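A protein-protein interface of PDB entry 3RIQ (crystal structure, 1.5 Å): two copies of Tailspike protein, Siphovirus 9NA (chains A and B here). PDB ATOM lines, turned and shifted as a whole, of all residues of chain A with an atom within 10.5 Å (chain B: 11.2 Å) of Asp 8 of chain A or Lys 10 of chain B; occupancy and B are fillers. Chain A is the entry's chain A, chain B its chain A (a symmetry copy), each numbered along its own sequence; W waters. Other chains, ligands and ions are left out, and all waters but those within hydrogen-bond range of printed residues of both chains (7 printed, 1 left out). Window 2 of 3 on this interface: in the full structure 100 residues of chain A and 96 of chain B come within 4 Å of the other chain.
NZ of Lys 10 of chain B lies within salt-bridge range of OD1 of Asp 8 of chain A, 2.7 Å away. N of Lys 12 of chain B is in hydrogen-bond range of O of Lys 12 of chain A, at 2.9 Å. O of Lys 10 of chain B is in hydrogen-bond range of N of Ser 14 of chain A (2.9 Å). The backbone carbonyl oxygen of Ser 14 of chain A lies within hydrogen-bond range of the backbone NH of Phe 11 of chain B (3.4 Å). The side-chain amino group (NZ) of Lys 16 of chain A sits at hydrogen-bond distance from the backbone carbonyl oxygen (O) of Asp 8 of chain B, at 2.7 Å.
N of Ser 5 of chain A lies within hydrogen-bond range of OD2 of Asp 8 of chain A, 2.9 Å away. The side-chain amino group (NZ) of Lys 16 of chain A lies within salt-bridge range of the side-chain carboxylate (OD2) of Asp 19 of chain A (2.8 Å). The side-chain amino group (NZ) of Lys 12 of chain B lies within salt-bridge range of the side-chain carboxylate (OD2) of Asp 32 of chain B (2.8 Å).
Phe 11 of chain B touches Ala 7 of chain A (CZ to O, 3.8 Å). OD1 of Asp 8 of chain A touches CZ of Phe 11 of chain B, at 3.5 Å. Phe 11 of chain A touches Phe 11 of chain B (CB to CD1, 3.6 Å). Lys 10 of chain B touches Tyr 13 of chain A (O to CA, 3.3 Å). CE1 of Tyr 13 of chain A touches CE1 of Phe 11 of chain B (3.9 Å). O of Ser 14 of chain A touches O of Lys 9 of chain B, 3.6 Å away. Lys 9 of chain B touches Asp 19 of chain A. Leu 35 of chain A touches Asp 32 of chain B (CD2 to OD2, 3.5 Å).
No residue of chain B comes within 4 Å of Phe 3 of chain A. No residue of chain B comes within 4 Å of Arg 4 of chain A. Of chain B, only Phe 11 comes within 4 Å of Ala 7 of chain A. Of the printed residues of chain B, Asp 8 of chain A touches Lys 10 (2.7 Å) and Phe 11 (3.5 Å). Printed residues of chain B within 4 Å of Phe 11 of chain A: Phe 11. Ser 14 of chain A touches four residues of chain B. Of the printed residues of chain B, Lys 16 of chain A touches Asp 8 (2.7 Å) and Tyr 13 (3.9 Å). Of the printed residues of chain A, Lys 9 of chain B touches Ser 14 (3.6 Å), Val 15 (3.7 Å) and Asp 19 (3.6 Å). Lys 10 of chain B touches three residues of chain A. Of chain A, only Ala 7 (3.8 Å), Asp 8 (3.5 Å), Phe 11 (3.6 Å), Lys 12 (3.2 Å), Tyr 13 (3.9 Å) and Ser 14 (3.4 Å) come within 4 Å of Phe 11 of chain B. Of the printed residues of chain A, Tyr 13 of chain B touches Lys 16. The nearest printed residue of chain B that does not touch Leu 35 of chain A is Lys 12 of chain B (4.4 Å).
Among the printed residues, Asp or Glu carboxylates within 4 Å of a Lys or Arg side-chain nitrogen of the other chain: Asp 8 of chain A with Lys 10 of chain B (2.7 Å).
Lys 12 of chain A touches Phe 11 of chain B, but with the chains exchanged Phe 11 of chain A does not touch Lys 12 of chain B (5.9 Å). Lys 12 of chain A touches its own counterpart, Lys 12 of chain B. Ser 14 of chain A touches Lys 12 of chain B, but with the chains exchanged Lys 12 of chain A does not touch Ser 14 of chain B (7.5 Å). Positions printed for both chains: 4, 5, 6, 7, 8, 9, 10, 11, 12, 13, 14 and 32.
Water W3 lies within hydrogen-bond range of the side-chain carboxylate (OD2) of Asp 19 of chain A (2.7 Å), the backbone carbonyl oxygen (O) of Lys 9 of chain B (2.7 Å), the side-chain hydroxyl (OH) of Tyr 20 of chain A (2.9 Å) and the backbone NH (N) of Lys 16 of chain A (3.0 Å). Water W1 lies within hydrogen-bond range of OH of Tyr 13 of chain A (2.8 Å) and NZ of Lys 10 of chain B (3.0 Å). Water W5 bridges OG of Ser 14 of chain A (2.8 Å) and NZ of Lys 12 of chain B (2.9 Å).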
ATOM      1  N   PHE A   3       4.491  -0.999  42.186  1.00  0.00           N
ATOM      2  CA  PHE A   3       5.657  -1.895  42.466  1.00  0.00           C
ATOM      3  C   PHE A   3       6.817  -1.643  41.486  1.00  0.00           C
ATOM      4  O   PHE A   3       6.627  -1.591  40.260  1.00  0.00           O
ATOM      5  CB  PHE A   3       5.237  -3.380  42.474  1.00  0.00           C
ATOM      6  CG  PHE A   3       6.366  -4.346  42.158  1.00  0.00           C
ATOM      7  CD1 PHE A   3       7.326  -4.652  43.123  1.00  0.00           C
ATOM      8  CD2 PHE A   3       6.447  -4.964  40.895  1.00  0.00           C
ATOM      9  CE1 PHE A   3       8.372  -5.542  42.843  1.00  0.00           C
ATOM     10  CE2 PHE A   3       7.478  -5.860  40.595  1.00  0.00           C
ATOM     11  CZ  PHE A   3       8.444  -6.152  41.588  1.00  0.00           C
ATOM     12  N   ARG A   4       8.009  -1.471  42.055  1.00  0.00           N
ATOM     13  CA  ARG A   4       9.259  -1.341  41.291  1.00  0.00           C
ATOM     14  C   ARG A   4      10.217  -2.395  41.826  1.00  0.00           C
ATOM     15  O   ARG A   4      10.492  -2.440  43.054  1.00  0.00           O
ATOM     16  CB  ARG A   4       9.867   0.075  41.455  1.00  0.00           C
ATOM     17  CG  ARG A   4       8.990   1.194  40.892  1.00  0.00           C
ATOM     18  N   SER A   5      10.718  -3.238  40.920  1.00  0.00           N
ATOM     19  CA  SER A   5      11.704  -4.282  41.273  1.00  0.00           C
ATOM     20  C   SER A   5      13.069  -3.640  41.508  1.00  0.00           C
ATOM     21  O   SER A   5      13.247  -2.431  41.278  1.00  0.00           O
ATOM     22  CB  SER A   5      11.838  -5.323  40.144  1.00  0.00           C
ATOM     23  OG  SER A   5      12.506  -4.732  39.033  1.00  0.00           O
ATOM     24  N   GLU A   6      14.038  -4.443  41.954  1.00  0.00           N
ATOM     25  CA  GLU A   6      15.375  -3.932  42.156  1.00  0.00           C
ATOM     26  C   GLU A   6      16.029  -3.450  40.856  1.00  0.00           C
ATOM     27  O   GLU A   6      16.726  -2.449  40.853  1.00  0.00           O
ATOM     28  CB  GLU A   6      16.250  -4.943  42.874  1.00  0.00           C
ATOM     29  CG  GLU A   6      15.834  -5.077  44.342  1.00  0.00           C
ATOM     30  CD  GLU A   6      16.845  -5.846  45.205  1.00  0.00           C
ATOM     31  OE1 GLU A   6      16.608  -7.065  45.484  1.00  0.00           O
ATOM     32  OE2 GLU A   6      17.868  -5.231  45.609  1.00  0.00           O
ATOM     33  N   ALA A   7      15.792  -4.137  39.740  1.00  0.00           N
ATOM     34  CA  ALA A   7      16.345  -3.653  38.468  1.00  0.00           C
ATOM     35  C   ALA A   7      15.762  -2.283  38.121  1.00  0.00           C
ATOM     36  O   ALA A   7      16.476  -1.392  37.645  1.00  0.00           O
ATOM     37  CB  ALA A   7      16.049  -4.634  37.335  1.00  0.00           C
ATOM     38  N   ASP A   8      14.457  -2.120  38.379  1.00  0.00           N
ATOM     39  CA  ASP A   8      13.779  -0.851  38.106  1.00  0.00           C
ATOM     40  C   ASP A   8      14.446   0.312  38.833  1.00  0.00           C
ATOM     41  O   ASP A   8      14.375   1.473  38.377  1.00  0.00           O
ATOM     42  CB  ASP A   8      12.298  -0.900  38.565  1.00  0.00           C
ATOM     43  CG  ASP A   8      11.426  -1.869  37.752  1.00  0.00           C
ATOM     44  OD1 ASP A   8      11.828  -2.293  36.660  1.00  0.00           O
ATOM     45  OD2 ASP A   8      10.303  -2.191  38.219  1.00  0.00           O
ATOM     46  N   LYS A   9      15.065   0.033  39.981  1.00  0.00           N
ATOM     47  CA  LYS A   9      15.675   1.100  40.771  1.00  0.00           C
ATOM     48  C   LYS A   9      17.120   1.409  40.395  1.00  0.00           C
ATOM     49  O   LYS A   9      17.665   2.403  40.852  1.00  0.00           O
ATOM     50  CB  LYS A   9      15.582   0.814  42.280  1.00  0.00           C
ATOM     51  CG  LYS A   9      14.115   0.788  42.756  1.00  0.00           C
ATOM     52  CD  LYS A   9      13.968   0.624  44.235  1.00  0.00           C
ATOM     53  CE  LYS A   9      12.532   0.249  44.531  1.00  0.00           C
ATOM     54  NZ  LYS A   9      12.249   0.242  45.992  1.00  0.00           N
ATOM     55  N   LYS A  10      17.745   0.582  39.574  1.00  0.00           N
ATOM     56  CA  LYS A  10      19.151   0.821  39.269  1.00  0.00           C
ATOM     57  C   LYS A  10      19.467   1.132  37.815  1.00  0.00           C
ATOM     58  O   LYS A  10      20.588   1.547  37.526  1.00  0.00           O
ATOM     59  CB  LYS A  10      20.029  -0.342  39.740  1.00  0.00           C
ATOM     60  CG  LYS A  10      19.853  -1.604  38.982  1.00  0.00           C
ATOM     61  CD  LYS A  10      20.640  -2.760  39.616  1.00  0.00           C
ATOM     62  CE  LYS A  10      22.159  -2.605  39.584  1.00  0.00           C
ATOM     63  NZ  LYS A  10      22.798  -3.921  39.963  1.00  0.00           N
ATOM     64  N   PHE A  11      18.507   0.939  36.912  1.00  0.00           N
ATOM     65  CA  PHE A  11      18.783   1.128  35.470  1.00  0.00           C
ATOM     66  C   PHE A  11      17.932   2.238  34.852  1.00  0.00           C
ATOM     67  O   PHE A  11      16.789   2.512  35.283  1.00  0.00           O
ATOM     68  CB  PHE A  11      18.504  -0.150  34.694  1.00  0.00           C
ATOM     69  CG  PHE A  11      19.369  -1.316  35.103  1.00  0.00           C
ATOM     70  CD1 PHE A  11      20.755  -1.170  35.235  1.00  0.00           C
ATOM     71  CD2 PHE A  11      18.803  -2.575  35.318  1.00  0.00           C
ATOM     72  CE1 PHE A  11      21.550  -2.302  35.592  1.00  0.00           C
ATOM     73  CE2 PHE A  11      19.574  -3.657  35.700  1.00  0.00           C
ATOM     74  CZ  PHE A  11      20.963  -3.520  35.832  1.00  0.00           C
ATOM     75  N   LYS A  12      18.529   2.924  33.888  1.00  0.00           N
ATOM     76  CA  LYS A  12      17.859   4.003  33.165  1.00  0.00           C
ATOM     77  C   LYS A  12      16.710   3.481  32.285  1.00  0.00           C
ATOM     78  O   LYS A  12      16.897   2.529  31.542  1.00  0.00           O
ATOM     79  CB  LYS A  12      18.929   4.640  32.255  1.00  0.00           C
ATOM     80  CG  LYS A  12      18.460   5.735  31.341  1.00  0.00           C
ATOM     81  CD  LYS A  12      18.298   7.018  32.064  1.00  0.00           C
ATOM     82  CE  LYS A  12      18.190   8.212  31.061  1.00  0.00           C
ATOM     83  NZ  LYS A  12      17.821   9.432  31.785  1.00  0.00           N
ATOM     84  N   TYR A  13      15.537   4.105  32.360  1.00  0.00           N
ATOM     85  CA  TYR A  13      14.415   3.751  31.490  1.00  0.00           C
ATOM     86  C   TYR A  13      14.572   4.306  30.094  1.00  0.00           C
ATOM     87  O   TYR A  13      14.727   5.531  29.902  1.00  0.00           O
ATOM     88  CB  TYR A  13      13.103   4.255  32.083  1.00  0.00           C
ATOM     89  CG  TYR A  13      12.560   3.402  33.248  1.00  0.00           C
ATOM     90  CD1 TYR A  13      13.331   3.112  34.393  1.00  0.00           C
ATOM     91  CD2 TYR A  13      11.297   2.868  33.170  1.00  0.00           C
ATOM     92  CE1 TYR A  13      12.817   2.308  35.444  1.00  0.00           C
ATOM     93  CE2 TYR A  13      10.780   2.073  34.176  1.00  0.00           C
ATOM     94  CZ  TYR A  13      11.520   1.800  35.312  1.00  0.00           C
ATOM     95  OH  TYR A  13      10.912   1.031  36.267  1.00  0.00           O
ATOM     96  N   SER A  14      14.525   3.399  29.115  1.00  0.00           N
ATOM     97  CA  SER A  14      14.511   3.780  27.710  1.00  0.00           C
ATOM     98  C   SER A  14      13.718   2.738  26.952  1.00  0.00           C
ATOM     99  O   SER A  14      13.833   1.529  27.239  1.00  0.00           O
ATOM    100  CB  SER A  14      15.948   3.882  27.165  1.00  0.00           C
ATOM    101  OG  SER A  14      15.916   4.294  25.810  1.00  0.00           O
ATOM    102  N   VAL A  15      12.902   3.205  26.019  1.00  0.00           N
ATOM    103  CA  VAL A  15      12.281   2.310  25.054  1.00  0.00           C
ATOM    104  C   VAL A  15      12.851   2.616  23.689  1.00  0.00           C
ATOM    105  O   VAL A  15      13.326   3.741  23.451  1.00  0.00           O
ATOM    106  CB  VAL A  15      10.740   2.474  24.998  1.00  0.00           C
ATOM    107  CG1 VAL A  15      10.095   2.076  26.353  1.00  0.00           C
ATOM    108  CG2 VAL A  15      10.356   3.865  24.541  1.00  0.00           C
ATOM    109  N   LYS A  16      12.811   1.645  22.785  1.00  0.00           N
ATOM    110  CA  LYS A  16      13.378   1.859  21.450  1.00  0.00           C
ATOM    111  C   LYS A  16      12.366   1.563  20.377  1.00  0.00           C
ATOM    112  O   LYS A  16      11.588   0.595  20.480  1.00  0.00           O
ATOM    113  CB  LYS A  16      14.676   1.058  21.242  1.00  0.00           C
ATOM    114  CG  LYS A  16      14.427  -0.438  21.290  1.00  0.00           C
ATOM    115  CD  LYS A  16      15.722  -1.253  21.322  1.00  0.00           C
ATOM    116  CE  LYS A  16      16.114  -1.587  22.721  1.00  0.00           C
ATOM    117  NZ  LYS A  16      15.204  -2.562  23.403  1.00  0.00           N
ATOM    118  N   LEU A  17      12.394   2.372  19.318  1.00  0.00           N
ATOM    119  CA  LEU A  17      11.399   2.266  18.263  1.00  0.00           C
ATOM    120  C   LEU A  17      11.327   0.870  17.642  1.00  0.00           C
ATOM    121  O   LEU A  17      10.231   0.434  17.268  1.00  0.00           O
ATOM    122  CB  LEU A  17      11.656   3.323  17.184  1.00  0.00           C
ATOM    123  CG  LEU A  17      10.656   3.356  16.006  1.00  0.00           C
ATOM    124  CD1 LEU A  17       9.216   3.608  16.483  1.00  0.00           C
ATOM    125  CD2 LEU A  17      11.091   4.477  15.058  1.00  0.00           C
ATOM    126  N   ASP A  19      11.277  -1.911  18.837  1.00  0.00           N
ATOM    127  CA  ASP A  19      10.431  -2.847  19.594  1.00  0.00           C
ATOM    128  C   ASP A  19       8.924  -2.695  19.264  1.00  0.00           C
ATOM    129  O   ASP A  19       8.097  -3.446  19.789  1.00  0.00           O
ATOM    130  CB  ASP A  19      10.659  -2.631  21.093  1.00  0.00           C
ATOM    131  CG  ASP A  19      11.958  -3.246  21.590  1.00  0.00           C
ATOM    132  OD1 ASP A  19      12.454  -4.253  20.991  1.00  0.00           O
ATOM    133  OD2 ASP A  19      12.469  -2.755  22.637  1.00  0.00           O
ATOM    134  N   TYR A  20       8.576  -1.714  18.427  1.00  0.00           N
ATOM    135  CA  TYR A  20       7.159  -1.362  18.134  1.00  0.00           C
ATOM    136  C   TYR A  20       6.901  -1.244  16.635  1.00  0.00           C
ATOM    137  O   TYR A  20       7.834  -1.098  15.834  1.00  0.00           O
ATOM    138  CB  TYR A  20       6.732  -0.064  18.856  1.00  0.00           C
ATOM    139  CG  TYR A  20       7.154  -0.103  20.301  1.00  0.00           C
ATOM    140  CD1 TYR A  20       6.354  -0.720  21.262  1.00  0.00           C
ATOM    141  CD2 TYR A  20       8.399   0.389  20.691  1.00  0.00           C
ATOM    142  CE1 TYR A  20       6.769  -0.826  22.574  1.00  0.00           C
ATOM    143  CE2 TYR A  20       8.826   0.285  22.008  1.00  0.00           C
ATOM    144  CZ  TYR A  20       8.020  -0.343  22.942  1.00  0.00           C
ATOM    145  OH  TYR A  20       8.482  -0.466  24.245  1.00  0.00           O
ATOM    146  N   ALA A  26       5.597   3.388  20.631  1.00  0.00           N
ATOM    147  CA  ALA A  26       6.846   3.655  21.352  1.00  0.00           C
ATOM    148  C   ALA A  26       6.665   4.816  22.359  1.00  0.00           C
ATOM    149  O   ALA A  26       7.100   4.717  23.511  1.00  0.00           O
ATOM    150  CB  ALA A  26       7.980   3.952  20.352  1.00  0.00           C
ATOM    151  N   ALA A  29       4.735   3.716  25.442  1.00  0.00           N
ATOM    152  CA  ALA A  29       5.542   2.889  26.342  1.00  0.00           C
ATOM    153  C   ALA A  29       6.598   3.720  27.087  1.00  0.00           C
ATOM    154  O   ALA A  29       7.024   3.334  28.165  1.00  0.00           O
ATOM    155  CB  ALA A  29       6.228   1.800  25.545  1.00  0.00           C
ATOM    156  N   ALA A  30       7.023   4.843  26.498  1.00  0.00           N
ATOM    157  CA  ALA A  30       8.139   5.630  27.041  1.00  0.00           C
ATOM    158  C   ALA A  30       7.864   6.220  28.407  1.00  0.00           C
ATOM    159  O   ALA A  30       6.739   6.588  28.727  1.00  0.00           O
ATOM    160  CB  ALA A  30       8.514   6.758  26.029  1.00  0.00           C
ATOM    161  N   VAL A  31       8.907   6.280  29.229  1.00  0.00           N
ATOM    162  CA  VAL A  31       8.856   6.891  30.564  1.00  0.00           C
ATOM    163  C   VAL A  31       9.858   8.036  30.710  1.00  0.00           C
ATOM    164  O   VAL A  31       9.537   9.129  31.209  1.00  0.00           O
ATOM    165  CB  VAL A  31       9.137   5.823  31.665  1.00  0.00           C
ATOM    166  CG1 VAL A  31       9.171   6.458  33.034  1.00  0.00           C
ATOM    167  CG2 VAL A  31       8.041   4.712  31.592  1.00  0.00           C
ATOM    168  N   ASP A  32      11.082   7.774  30.286  1.00  0.00           N
ATOM    169  CA  ASP A  32      12.204   8.727  30.458  1.00  0.00           C
ATOM    170  C   ASP A  32      12.801   8.983  29.065  1.00  0.00           C
ATOM    171  O   ASP A  32      12.678  10.073  28.523  1.00  0.00           O
ATOM    172  CB  ASP A  32      13.206   8.082  31.400  1.00  0.00           C
ATOM    173  CG  ASP A  32      14.474   8.912  31.631  1.00  0.00           C
ATOM    174  OD1 ASP A  32      14.668   9.965  30.982  1.00  0.00           O
ATOM    175  OD2 ASP A  32      15.321   8.457  32.439  1.00  0.00           O
ATOM    176  N   SER A  33      13.443   7.964  28.494  1.00  0.00           N
ATOM    177  CA  SER A  33      14.052   8.103  27.176  1.00  0.00           C
ATOM    178  C   SER A  33      13.360   7.280  26.089  1.00  0.00           C
ATOM    179  O   SER A  33      12.753   6.249  26.367  1.00  0.00           O
ATOM    180  CB  SER A  33      15.528   7.769  27.288  1.00  0.00           C
ATOM    181  OG  SER A  33      16.128   8.687  28.183  1.00  0.00           O
ATOM    182  N   LEU A  34      13.457   7.768  24.852  1.00  0.00           N
ATOM    183  CA  LEU A  34      12.869   7.150  23.670  1.00  0.00           C
ATOM    184  C   LEU A  34      13.965   7.155  22.621  1.00  0.00           C
ATOM    185  O   LEU A  34      14.405   8.231  22.202  1.00  0.00           O
ATOM    186  CB  LEU A  34      11.605   7.920  23.223  1.00  0.00           C
ATOM    187  CG  LEU A  34      11.100   7.631  21.797  1.00  0.00           C
ATOM    188  CD1 LEU A  34      10.851   6.150  21.540  1.00  0.00           C
ATOM    189  CD2 LEU A  34       9.852   8.484  21.562  1.00  0.00           C
ATOM    190  N   LEU A  35      14.442   5.974  22.243  1.00  0.00           N
ATOM    191  CA  LEU A  35      15.530   5.850  21.267  1.00  0.00           C
ATOM    192  C   LEU A  35      14.973   5.571  19.874  1.00  0.00           C
ATOM    193  O   LEU A  35      14.236   4.603  19.693  1.00  0.00           O
ATOM    194  CB  LEU A  35      16.501   4.735  21.704  1.00  0.00           C
ATOM    195  CG  LEU A  35      17.611   4.390  20.703  1.00  0.00           C
ATOM    196  CD1 LEU A  35      18.630   5.546  20.684  1.00  0.00           C
ATOM    197  CD2 LEU A  35      18.280   3.064  21.088  1.00  0.00           C
ATOM    198  N   ARG B   4      14.044 -10.700  22.791  1.00  0.00           N
ATOM    199  CA  ARG B   4      14.267  -9.600  23.743  1.00  0.00           C
ATOM    200  C   ARG B   4      13.333  -9.837  24.920  1.00  0.00           C
ATOM    201  O   ARG B   4      12.095  -9.970  24.732  1.00  0.00           O
ATOM    202  CB  ARG B   4      13.972  -8.229  23.086  1.00  0.00           C
ATOM    203  CG  ARG B   4      14.905  -7.886  21.924  1.00  0.00           C
ATOM    204  N   SER B   5      13.914  -9.894  26.120  1.00  0.00           N
ATOM    205  CA  SER B   5      13.137 -10.063  27.367  1.00  0.00           C
ATOM    206  C   SER B   5      12.431  -8.754  27.712  1.00  0.00           C
ATOM    207  O   SER B   5      12.652  -7.723  27.053  1.00  0.00           O
ATOM    208  CB  SER B   5      14.053 -10.453  28.543  1.00  0.00           C
ATOM    209  OG  SER B   5      14.851  -9.332  28.912  1.00  0.00           O
ATOM    210  N   GLU B   6      11.590  -8.785  28.749  1.00  0.00           N
ATOM    211  CA  GLU B   6      10.917  -7.580  29.179  1.00  0.00           C
ATOM    212  C   GLU B   6      11.888  -6.502  29.676  1.00  0.00           C
ATOM    213  O   GLU B   6      11.685  -5.327  29.421  1.00  0.00           O
ATOM    214  CB  GLU B   6       9.850  -7.883  30.215  1.00  0.00           C
ATOM    215  CG  GLU B   6       8.655  -8.594  29.572  1.00  0.00           C
ATOM    216  CD  GLU B   6       7.418  -8.669  30.479  1.00  0.00           C
ATOM    217  OE1 GLU B   6       7.174  -9.757  31.092  1.00  0.00           O
ATOM    218  OE2 GLU B   6       6.688  -7.645  30.571  1.00  0.00           O
ATOM    219  N   ALA B   7      12.960  -6.890  30.364  1.00  0.00           N
ATOM    220  CA  ALA B   7      13.944  -5.884  30.786  1.00  0.00           C
ATOM    221  C   ALA B   7      14.581  -5.217  29.566  1.00  0.00           C
ATOM    222  O   ALA B   7      14.798  -4.000  29.550  1.00  0.00           O
ATOM    223  CB  ALA B   7      15.036  -6.516  31.647  1.00  0.00           C
ATOM    224  N   ASP B   8      14.864  -6.028  28.536  1.00  0.00           N
ATOM    225  CA  ASP B   8      15.462  -5.514  27.304  1.00  0.00           C
ATOM    226  C   ASP B   8      14.611  -4.411  26.681  1.00  0.00           C
ATOM    227  O   ASP B   8      15.134  -3.529  25.969  1.00  0.00           O
ATOM    228  CB  ASP B   8      15.614  -6.638  26.246  1.00  0.00           C
ATOM    229  CG  ASP B   8      16.637  -7.718  26.630  1.00  0.00           C
ATOM    230  OD1 ASP B   8      17.456  -7.501  27.533  1.00  0.00           O
ATOM    231  OD2 ASP B   8      16.625  -8.801  25.989  1.00  0.00           O
ATOM    232  N   LYS B   9      13.296  -4.465  26.903  1.00  0.00           N
ATOM    233  CA  LYS B   9      12.403  -3.484  26.291  1.00  0.00           C
ATOM    234  C   LYS B   9      12.205  -2.217  27.117  1.00  0.00           C
ATOM    235  O   LYS B   9      11.638  -1.254  26.621  1.00  0.00           O
ATOM    236  CB  LYS B   9      11.035  -4.097  25.949  1.00  0.00           C
ATOM    237  CG  LYS B   9      11.168  -5.200  24.878  1.00  0.00           C
ATOM    238  CD  LYS B   9       9.855  -5.756  24.425  1.00  0.00           C
ATOM    239  CE  LYS B   9      10.120  -7.045  23.676  1.00  0.00           C
ATOM    240  NZ  LYS B   9       8.887  -7.576  23.033  1.00  0.00           N
ATOM    241  N   LYS B  10      12.662  -2.200  28.359  1.00  0.00           N
ATOM    242  CA  LYS B  10      12.409  -1.025  29.185  1.00  0.00           C
ATOM    243  C   LYS B  10      13.641  -0.259  29.635  1.00  0.00           C
ATOM    244  O   LYS B  10      13.497   0.848  30.153  1.00  0.00           O
ATOM    245  CB  LYS B  10      11.557  -1.378  30.408  1.00  0.00           C
ATOM    246  CG  LYS B  10      12.239  -2.216  31.423  1.00  0.00           C
ATOM    247  CD  LYS B  10      11.274  -2.662  32.531  1.00  0.00           C
ATOM    248  CE  LYS B  10      10.721  -1.535  33.402  1.00  0.00           C
ATOM    249  NZ  LYS B  10      10.037  -2.134  34.609  1.00  0.00           N
ATOM    250  N   PHE B  11      14.832  -0.824  29.448  1.00  0.00           N
ATOM    251  CA  PHE B  11      16.062  -0.173  29.954  1.00  0.00           C
ATOM    252  C   PHE B  11      17.034   0.193  28.833  1.00  0.00           C
ATOM    253  O   PHE B  11      17.102  -0.471  27.774  1.00  0.00           O
ATOM    254  CB  PHE B  11      16.800  -1.088  30.920  1.00  0.00           C
ATOM    255  CG  PHE B  11      16.010  -1.436  32.157  1.00  0.00           C
ATOM    256  CD1 PHE B  11      15.358  -0.442  32.897  1.00  0.00           C
ATOM    257  CD2 PHE B  11      15.951  -2.757  32.609  1.00  0.00           C
ATOM    258  CE1 PHE B  11      14.645  -0.801  34.082  1.00  0.00           C
ATOM    259  CE2 PHE B  11      15.227  -3.102  33.736  1.00  0.00           C
ATOM    260  CZ  PHE B  11      14.573  -2.113  34.483  1.00  0.00           C
ATOM    261  N   LYS B  12      17.732   1.301  29.042  1.00  0.00           N
ATOM    262  CA  LYS B  12      18.728   1.789  28.091  1.00  0.00           C
ATOM    263  C   LYS B  12      19.950   0.859  28.007  1.00  0.00           C
ATOM    264  O   LYS B  12      20.497   0.478  29.031  1.00  0.00           O
ATOM    265  CB  LYS B  12      19.189   3.164  28.620  1.00  0.00           C
ATOM    266  CG  LYS B  12      20.282   3.842  27.847  1.00  0.00           C
ATOM    267  CD  LYS B  12      19.766   4.478  26.613  1.00  0.00           C
ATOM    268  CE  LYS B  12      20.808   5.487  26.030  1.00  0.00           C
ATOM    269  NZ  LYS B  12      20.367   5.943  24.708  1.00  0.00           N
ATOM    270  N   TYR B  13      20.379   0.506  26.797  1.00  0.00           N
ATOM    271  CA  TYR B  13      21.593  -0.290  26.609  1.00  0.00           C
ATOM    272  C   TYR B  13      22.851   0.531  26.768  1.00  0.00           C
ATOM    273  O   TYR B  13      23.046   1.550  26.071  1.00  0.00           O
ATOM    274  CB  TYR B  13      21.593  -0.941  25.229  1.00  0.00           C
ATOM    275  CG  TYR B  13      20.679  -2.177  25.107  1.00  0.00           C
ATOM    276  CD1 TYR B  13      19.307  -2.136  25.434  1.00  0.00           C
ATOM    277  CD2 TYR B  13      21.208  -3.377  24.701  1.00  0.00           C
ATOM    278  CE1 TYR B  13      18.489  -3.291  25.332  1.00  0.00           C
ATOM    279  CE2 TYR B  13      20.433  -4.518  24.604  1.00  0.00           C
ATOM    280  CZ  TYR B  13      19.083  -4.484  24.903  1.00  0.00           C
ATOM    281  OH  TYR B  13      18.393  -5.655  24.748  1.00  0.00           O
ATOM    282  N   SER B  14      23.708   0.082  27.688  1.00  0.00           N
ATOM    283  CA  SER B  14      25.029   0.668  27.863  1.00  0.00           C
ATOM    284  C   SER B  14      25.966  -0.424  28.329  1.00  0.00           C
ATOM    285  O   SER B  14      25.578  -1.274  29.158  1.00  0.00           O
ATOM    286  CB  SER B  14      24.976   1.821  28.883  1.00  0.00           C
ATOM    287  OG  SER B  14      26.260   2.406  29.008  1.00  0.00           O
ATOM    288  N   ASP B  32      24.263   0.634  22.053  1.00  0.00           N
ATOM    289  CA  ASP B  32      23.730   2.017  22.046  1.00  0.00           C
ATOM    290  C   ASP B  32      24.793   2.918  22.695  1.00  0.00           C
ATOM    291  O   ASP B  32      25.411   3.736  22.026  1.00  0.00           O
ATOM    292  CB  ASP B  32      22.431   2.006  22.834  1.00  0.00           C
ATOM    293  CG  ASP B  32      21.779   3.385  22.987  1.00  0.00           C
ATOM    294  OD1 ASP B  32      22.369   4.413  22.582  1.00  0.00           O
ATOM    295  OD2 ASP B  32      20.677   3.438  23.587  1.00  0.00           O
HETATM  296  O   HOH W   1       8.377   0.058  35.730  1.00  0.00           O
HETATM  297  O   HOH W   2      11.362   2.663  29.566  1.00  0.00           O
HETATM  298  O   HOH W   3      11.344  -0.717  23.959  1.00  0.00           O
HETATM  299  O   HOH W   4      16.598  -4.891  22.779  1.00  0.00           O
HETATM  300  O   HOH W   5      17.498   6.294  24.597  1.00  0.00           O
HETATM  301  O   HOH W   6       8.408  -5.882  20.830  1.00  0.00           O
HETATM  302  O   HOH W   7       8.708  -4.160  37.127  1.00  0.00           O
